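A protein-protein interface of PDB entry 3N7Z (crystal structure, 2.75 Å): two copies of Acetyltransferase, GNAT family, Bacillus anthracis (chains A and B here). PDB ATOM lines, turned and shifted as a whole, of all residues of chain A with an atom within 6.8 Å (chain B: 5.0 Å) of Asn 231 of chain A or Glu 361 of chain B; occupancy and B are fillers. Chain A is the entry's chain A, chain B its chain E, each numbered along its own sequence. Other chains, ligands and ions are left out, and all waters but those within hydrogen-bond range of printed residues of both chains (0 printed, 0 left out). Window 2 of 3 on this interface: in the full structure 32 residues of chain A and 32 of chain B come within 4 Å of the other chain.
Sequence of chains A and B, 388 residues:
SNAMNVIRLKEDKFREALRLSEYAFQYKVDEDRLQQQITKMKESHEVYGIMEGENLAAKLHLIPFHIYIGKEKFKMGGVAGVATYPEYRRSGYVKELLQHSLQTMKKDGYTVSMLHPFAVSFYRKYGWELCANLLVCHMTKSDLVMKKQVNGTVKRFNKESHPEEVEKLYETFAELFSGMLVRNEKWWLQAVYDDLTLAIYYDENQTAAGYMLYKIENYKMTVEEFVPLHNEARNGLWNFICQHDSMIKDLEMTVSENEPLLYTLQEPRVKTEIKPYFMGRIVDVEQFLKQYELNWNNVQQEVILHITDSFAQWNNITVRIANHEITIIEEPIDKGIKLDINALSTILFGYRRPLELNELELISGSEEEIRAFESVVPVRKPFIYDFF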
ATOM      1  N   LYS A 147      27.350  17.676  11.176  1.00  0.00           N
ATOM      2  CA  LYS A 147      26.528  17.996  12.332  1.00  0.00           C
ATOM      3  C   LYS A 147      27.081  19.310  12.866  1.00  0.00           C
ATOM      4  O   LYS A 147      28.118  19.770  12.378  1.00  0.00           O
ATOM      5  CB  LYS A 147      26.602  16.873  13.363  1.00  0.00           C
ATOM      6  CG  LYS A 147      26.059  15.555  12.835  1.00  0.00           C
ATOM      7  CD  LYS A 147      26.264  14.405  13.820  1.00  0.00           C
ATOM      8  CE  LYS A 147      25.677  13.099  13.278  1.00  0.00           C
ATOM      9  NZ  LYS A 147      24.283  13.305  12.774  1.00  0.00           N
ATOM     10  N   VAL A 150      31.859  20.967  16.765  1.00  0.00           N
ATOM     11  CA  VAL A 150      32.311  20.768  18.138  1.00  0.00           C
ATOM     12  C   VAL A 150      33.678  21.429  18.332  1.00  0.00           C
ATOM     13  O   VAL A 150      34.404  21.671  17.363  1.00  0.00           O
ATOM     14  CB  VAL A 150      32.297  19.265  18.564  1.00  0.00           C
ATOM     15  CG1 VAL A 150      30.869  18.722  18.582  1.00  0.00           C
ATOM     16  CG2 VAL A 150      33.185  18.415  17.664  1.00  0.00           C
ATOM     17  N   PRO A 228      33.096   6.282  20.118  1.00  0.00           N
ATOM     18  CA  PRO A 228      32.984   7.554  20.816  1.00  0.00           C
ATOM     19  C   PRO A 228      32.595   7.300  22.269  1.00  0.00           C
ATOM     20  O   PRO A 228      31.934   6.306  22.542  1.00  0.00           O
ATOM     21  CB  PRO A 228      31.832   8.231  20.089  1.00  0.00           C
ATOM     22  CG  PRO A 228      30.949   7.118  19.676  1.00  0.00           C
ATOM     23  CD  PRO A 228      31.812   5.875  19.526  1.00  0.00           C
ATOM     24  N   LEU A 229      32.990   8.175  23.193  1.00  0.00           N
ATOM     25  CA  LEU A 229      32.636   7.978  24.599  1.00  0.00           C
ATOM     26  C   LEU A 229      31.350   8.681  24.953  1.00  0.00           C
ATOM     27  O   LEU A 229      30.719   8.354  25.951  1.00  0.00           O
ATOM     28  CB  LEU A 229      33.744   8.438  25.551  1.00  0.00           C
ATOM     29  CG  LEU A 229      35.067   7.664  25.645  1.00  0.00           C
ATOM     30  CD1 LEU A 229      35.662   7.962  26.992  1.00  0.00           C
ATOM     31  CD2 LEU A 229      34.952   6.140  25.398  1.00  0.00           C
ATOM     32  N   HIS A 230      30.988   9.664  24.145  1.00  0.00           N
ATOM     33  CA  HIS A 230      29.783  10.456  24.338  1.00  0.00           C
ATOM     34  C   HIS A 230      29.459  11.151  23.026  1.00  0.00           C
ATOM     35  O   HIS A 230      30.200  11.017  22.035  1.00  0.00           O
ATOM     36  CB  HIS A 230      29.962  11.493  25.448  1.00  0.00           C
ATOM     37  CG  HIS A 230      31.257  12.242  25.379  1.00  0.00           C
ATOM     38  ND1 HIS A 230      31.698  12.872  24.231  1.00  0.00           N
ATOM     39  CD2 HIS A 230      32.204  12.473  26.322  1.00  0.00           C
ATOM     40  CE1 HIS A 230      32.865  13.445  24.469  1.00  0.00           C
ATOM     41  NE2 HIS A 230      33.195  13.216  25.729  1.00  0.00           N
ATOM     42  N   ASN A 231      28.368  11.907  23.020  1.00  0.00           N
ATOM     43  CA  ASN A 231      27.855  12.444  21.783  1.00  0.00           C
ATOM     44  C   ASN A 231      28.783  13.434  21.125  1.00  0.00           C
ATOM     45  O   ASN A 231      28.895  13.445  19.905  1.00  0.00           O
ATOM     46  CB  ASN A 231      26.481  13.055  21.972  1.00  0.00           C
ATOM     47  CG  ASN A 231      25.745  13.183  20.678  1.00  0.00           C
ATOM     48  OD1 ASN A 231      25.796  12.288  19.836  1.00  0.00           O
ATOM     49  ND2 ASN A 231      25.065  14.299  20.494  1.00  0.00           N
ATOM     50  N   GLU A 232      29.445  14.263  21.930  1.00  0.00           N
ATOM     51  CA  GLU A 232      30.404  15.229  21.400  1.00  0.00           C
ATOM     52  C   GLU A 232      31.480  14.526  20.575  1.00  0.00           C
ATOM     53  O   GLU A 232      31.785  14.960  19.465  1.00  0.00           O
ATOM     54  CB  GLU A 232      31.041  16.088  22.492  1.00  0.00           C
ATOM     55  CG  GLU A 232      31.887  17.225  21.914  1.00  0.00           C
ATOM     56  CD  GLU A 232      32.865  17.847  22.907  1.00  0.00           C
ATOM     57  OE1 GLU A 232      32.418  18.241  24.005  1.00  0.00           O
ATOM     58  OE2 GLU A 232      34.077  17.959  22.578  1.00  0.00           O
ATOM     59  N   ALA A 233      32.039  13.436  21.092  1.00  0.00           N
ATOM     60  CA  ALA A 233      33.034  12.680  20.319  1.00  0.00           C
ATOM     61  C   ALA A 233      32.438  11.965  19.097  1.00  0.00           C
ATOM     62  O   ALA A 233      33.159  11.662  18.142  1.00  0.00           O
ATOM     63  CB  ALA A 233      33.776  11.704  21.206  1.00  0.00           C
ATOM     64  N   ARG A 234      31.131  11.691  19.133  1.00  0.00           N
ATOM     65  CA  ARG A 234      30.434  11.082  18.001  1.00  0.00           C
ATOM     66  C   ARG A 234      30.295  12.088  16.870  1.00  0.00           C
ATOM     67  O   ARG A 234      30.607  11.789  15.732  1.00  0.00           O
ATOM     68  CB  ARG A 234      29.064  10.549  18.416  1.00  0.00           C
ATOM     69  CG  ARG A 234      28.208  10.076  17.250  1.00  0.00           C
ATOM     70  CD  ARG A 234      26.910   9.499  17.714  1.00  0.00           C
ATOM     71  NE  ARG A 234      27.146   8.311  18.520  1.00  0.00           N
ATOM     72  CZ  ARG A 234      26.941   8.223  19.832  1.00  0.00           C
ATOM     73  NH1 ARG A 234      26.465   9.256  20.533  1.00  0.00           N
ATOM     74  NH2 ARG A 234      27.209   7.078  20.444  1.00  0.00           N
ATOM     75  N   ASN A 235      29.827  13.285  17.189  1.00  0.00           N
ATOM     76  CA  ASN A 235      29.832  14.376  16.234  1.00  0.00           C
ATOM     77  C   ASN A 235      31.234  14.723  15.759  1.00  0.00           C
ATOM     78  O   ASN A 235      31.456  14.954  14.570  1.00  0.00           O
ATOM     79  CB  ASN A 235      29.163  15.596  16.848  1.00  0.00           C
ATOM     80  CG  ASN A 235      27.669  15.400  17.032  1.00  0.00           C
ATOM     81  OD1 ASN A 235      27.159  14.282  16.933  1.00  0.00           O
ATOM     82  ND2 ASN A 235      26.960  16.487  17.293  1.00  0.00           N
ATOM     83  N   GLY A 236      32.175  14.735  16.695  1.00  0.00           N
ATOM     84  CA  GLY A 236      33.564  15.045  16.401  1.00  0.00           C
ATOM     85  C   GLY A 236      34.111  14.151  15.317  1.00  0.00           C
ATOM     86  O   GLY A 236      34.618  14.643  14.294  1.00  0.00           O
ATOM     87  N   LEU A 237      33.997  12.836  15.531  1.00  0.00           N
ATOM     88  CA  LEU A 237      34.478  11.858  14.547  1.00  0.00           C
ATOM     89  C   LEU A 237      33.637  11.883  13.268  1.00  0.00           C
ATOM     90  O   LEU A 237      34.179  11.760  12.165  1.00  0.00           O
ATOM     91  CB  LEU A 237      34.515  10.441  15.113  1.00  0.00           C
ATOM     92  CG  LEU A 237      35.314  10.064  16.364  1.00  0.00           C
ATOM     93  CD1 LEU A 237      34.908   8.651  16.753  1.00  0.00           C
ATOM     94  CD2 LEU A 237      36.819  10.160  16.186  1.00  0.00           C
ATOM     95  N   THR A 264      20.621   9.652  13.536  1.00  0.00           N
ATOM     96  CA  THR A 264      20.868  11.086  13.443  1.00  0.00           C
ATOM     97  C   THR A 264      21.126  11.585  12.014  1.00  0.00           C
ATOM     98  O   THR A 264      21.267  12.791  11.793  1.00  0.00           O
ATOM     99  CB  THR A 264      22.043  11.498  14.346  1.00  0.00           C
ATOM    100  OG1 THR A 264      23.258  10.959  13.816  1.00  0.00           O
ATOM    101  CG2 THR A 264      21.848  10.990  15.762  1.00  0.00           C
ATOM    102  N   LEU B 357      18.055   8.329  23.351  1.00  0.00           N
ATOM    103  CA  LEU B 357      17.896   9.731  22.996  1.00  0.00           C
ATOM    104  C   LEU B 357      18.620  10.684  23.945  1.00  0.00           C
ATOM    105  O   LEU B 357      18.935  11.816  23.571  1.00  0.00           O
ATOM    106  CB  LEU B 357      16.418  10.088  22.921  1.00  0.00           C
ATOM    107  CG  LEU B 357      15.557   9.314  21.925  1.00  0.00           C
ATOM    108  CD1 LEU B 357      14.145   9.801  22.050  1.00  0.00           C
ATOM    109  CD2 LEU B 357      16.044   9.530  20.510  1.00  0.00           C
ATOM    110  N   ASN B 358      18.891  10.224  25.163  1.00  0.00           N
ATOM    111  CA  ASN B 358      19.689  10.982  26.121  1.00  0.00           C
ATOM    112  C   ASN B 358      21.174  10.973  25.753  1.00  0.00           C
ATOM    113  O   ASN B 358      21.841  12.003  25.796  1.00  0.00           O
ATOM    114  CB  ASN B 358      19.500  10.420  27.527  1.00  0.00           C
ATOM    115  CG  ASN B 358      20.219  11.227  28.563  1.00  0.00           C
ATOM    116  OD1 ASN B 358      20.048  12.431  28.632  1.00  0.00           O
ATOM    117  ND2 ASN B 358      21.037  10.576  29.370  1.00  0.00           N
ATOM    118  N   GLU B 359      21.680   9.791  25.401  1.00  0.00           N
ATOM    119  CA  GLU B 359      23.045   9.636  24.907  1.00  0.00           C
ATOM    120  C   GLU B 359      23.241  10.527  23.687  1.00  0.00           C
ATOM    121  O   GLU B 359      24.313  11.108  23.488  1.00  0.00           O
ATOM    122  CB  GLU B 359      23.327   8.165  24.562  1.00  0.00           C
ATOM    123  CG  GLU B 359      24.527   7.894  23.612  1.00  0.00           C
ATOM    124  CD  GLU B 359      25.917   8.169  24.234  1.00  0.00           C
ATOM    125  OE1 GLU B 359      26.008   8.464  25.455  1.00  0.00           O
ATOM    126  OE2 GLU B 359      26.929   8.082  23.491  1.00  0.00           O
ATOM    127  N   LEU B 360      22.181  10.634  22.894  1.00  0.00           N
ATOM    128  CA  LEU B 360      22.170  11.453  21.697  1.00  0.00           C
ATOM    129  C   LEU B 360      21.882  12.921  21.953  1.00  0.00           C
ATOM    130  O   LEU B 360      21.935  13.726  21.022  1.00  0.00           O
ATOM    131  CB  LEU B 360      21.127  10.929  20.727  1.00  0.00           C
ATOM    132  CG  LEU B 360      21.449   9.677  19.941  1.00  0.00           C
ATOM    133  CD1 LEU B 360      20.238   9.385  19.086  1.00  0.00           C
ATOM    134  CD2 LEU B 360      22.679   9.900  19.108  1.00  0.00           C
ATOM    135  N   GLU B 361      21.556  13.266  23.197  1.00  0.00           N
ATOM    136  CA  GLU B 361      21.393  14.663  23.615  1.00  0.00           C
ATOM    137  C   GLU B 361      20.125  15.310  23.084  1.00  0.00           C
ATOM    138  O   GLU B 361      20.044  16.530  22.991  1.00  0.00           O
ATOM    139  CB  GLU B 361      22.617  15.495  23.223  1.00  0.00           C
ATOM    140  CG  GLU B 361      23.760  15.389  24.214  1.00  0.00           C
ATOM    141  CD  GLU B 361      25.052  16.043  23.736  1.00  0.00           C
ATOM    142  OE1 GLU B 361      25.106  16.602  22.617  1.00  0.00           O
ATOM    143  OE2 GLU B 361      26.035  15.989  24.497  1.00  0.00           O
ATOM    144  N   LEU B 362      19.130  14.496  22.749  1.00  0.00           N
ATOM    145  CA  LEU B 362      17.877  15.013  22.197  1.00  0.00           C
ATOM    146  C   LEU B 362      16.786  15.118  23.260  1.00  0.00           C
ATOM    147  O   LEU B 362      15.715  15.681  23.011  1.00  0.00           O
ATOM    148  CB  LEU B 362      17.403  14.173  21.001  1.00  0.00           C
ATOM    149  CG  LEU B 362      18.405  13.856  19.877  1.00  0.00           C
ATOM    150  CD1 LEU B 362      17.905  12.676  19.040  1.00  0.00           C
ATOM    151  CD2 LEU B 362      18.728  15.078  18.978  1.00  0.00           C
ATOM    152  N   ILE B 363      17.039  14.550  24.429  1.00  0.00           N
ATOM    153  CA  ILE B 363      16.222  14.833  25.601  1.00  0.00           C
ATOM    154  C   ILE B 363      17.194  15.154  26.730  1.00  0.00           C
ATOM    155  O   ILE B 363      18.363  14.753  26.659  1.00  0.00           O
ATOM    156  CB  ILE B 363      15.239  13.684  25.971  1.00  0.00           C
ATOM    157  CG1 ILE B 363      15.964  12.492  26.615  1.00  0.00           C
ATOM    158  CG2 ILE B 363      14.447  13.263  24.755  1.00  0.00           C
ATOM    159  CD1 ILE B 363      15.050  11.438  27.235  1.00  0.00           C
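ND2 of Asn 231 of chain A lies within hydrogen-bond range of O of Leu 360 of chain B (3.2 Å).
The side-chain carboxylate (OE1) of Glu 361 of chain B is in hydrogen-bond range of the side-chain amide nitrogen (ND2) of Asn 231 of chain A (3.1 Å).
The guanidinium group (NH1) of Arg 234 of chain A lies within salt-bridge range of the side-chain carboxylate (OE2) of Glu 359 of chain B (3.2 Å).
The side-chain amino group of Lys 147 of chain A is in hydrogen-bond range of the side-chain hydroxyl of Thr 264 of chain A (2.8 Å).
A ring nitrogen (ND1) of His 230 of chain A sits at hydrogen-bond distance from the backbone NH (N) of Ala 233 of chain A, at 3.2 Å.
OD1 of Asn 231 of chain A lies within hydrogen-bond range of NH1 of Arg 234 of chain A (3.2 Å).
Among the printed residues, pairs that only touch across the chains: Asn 231 of chain A with Glu 359 of chain B, Thr 264 of chain A with Leu 360 of chain B and His 230 of chain A with Glu 359 of chain B.
Pro 228 of chain A touches none of the printed residues of chain B.
Asn 231 of chain A touches just these residues of chain B: Glu 359, Leu 360 and Glu 361.
Of the printed residues of chain B, Arg 234 of chain A touches Glu 359 (3.2 Å).
Gly 236 of chain A touches none of the printed residues of chain B.
Printed residues of chain B within 4 Å of Thr 264 of chain A: Leu 360 (3.6 Å).
Of the printed residues of chain A, Glu 359 of chain B touches His 230, Asn 231 and Arg 234.
Printed residues of chain A within 4 Å of Leu 360 of chain B: Asn 231 (3.2 Å) and Thr 264 (3.6 Å).
Glu 361 of chain B touches just one residue of chain A: Asn 231.
The nearest printed residue of chain B that does not touch His 230 of chain A is Glu 361 of chain B (6.0 Å).
Of the 13 printed residues of chain A, 4 touch a printed residue of chain B.
Along chain A the printed residues that touch a printed residue of chain B span positions 230 to 264.
Among the printed residues, 6 pairs touch across the chains.
Among the printed residues, Asp or Glu carboxylates within 4 Å of a Lys or Arg side-chain nitrogen of the other chain: Arg 234 of chain A with Glu 359 of chain B (3.2 Å).
No position is printed for both chains.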
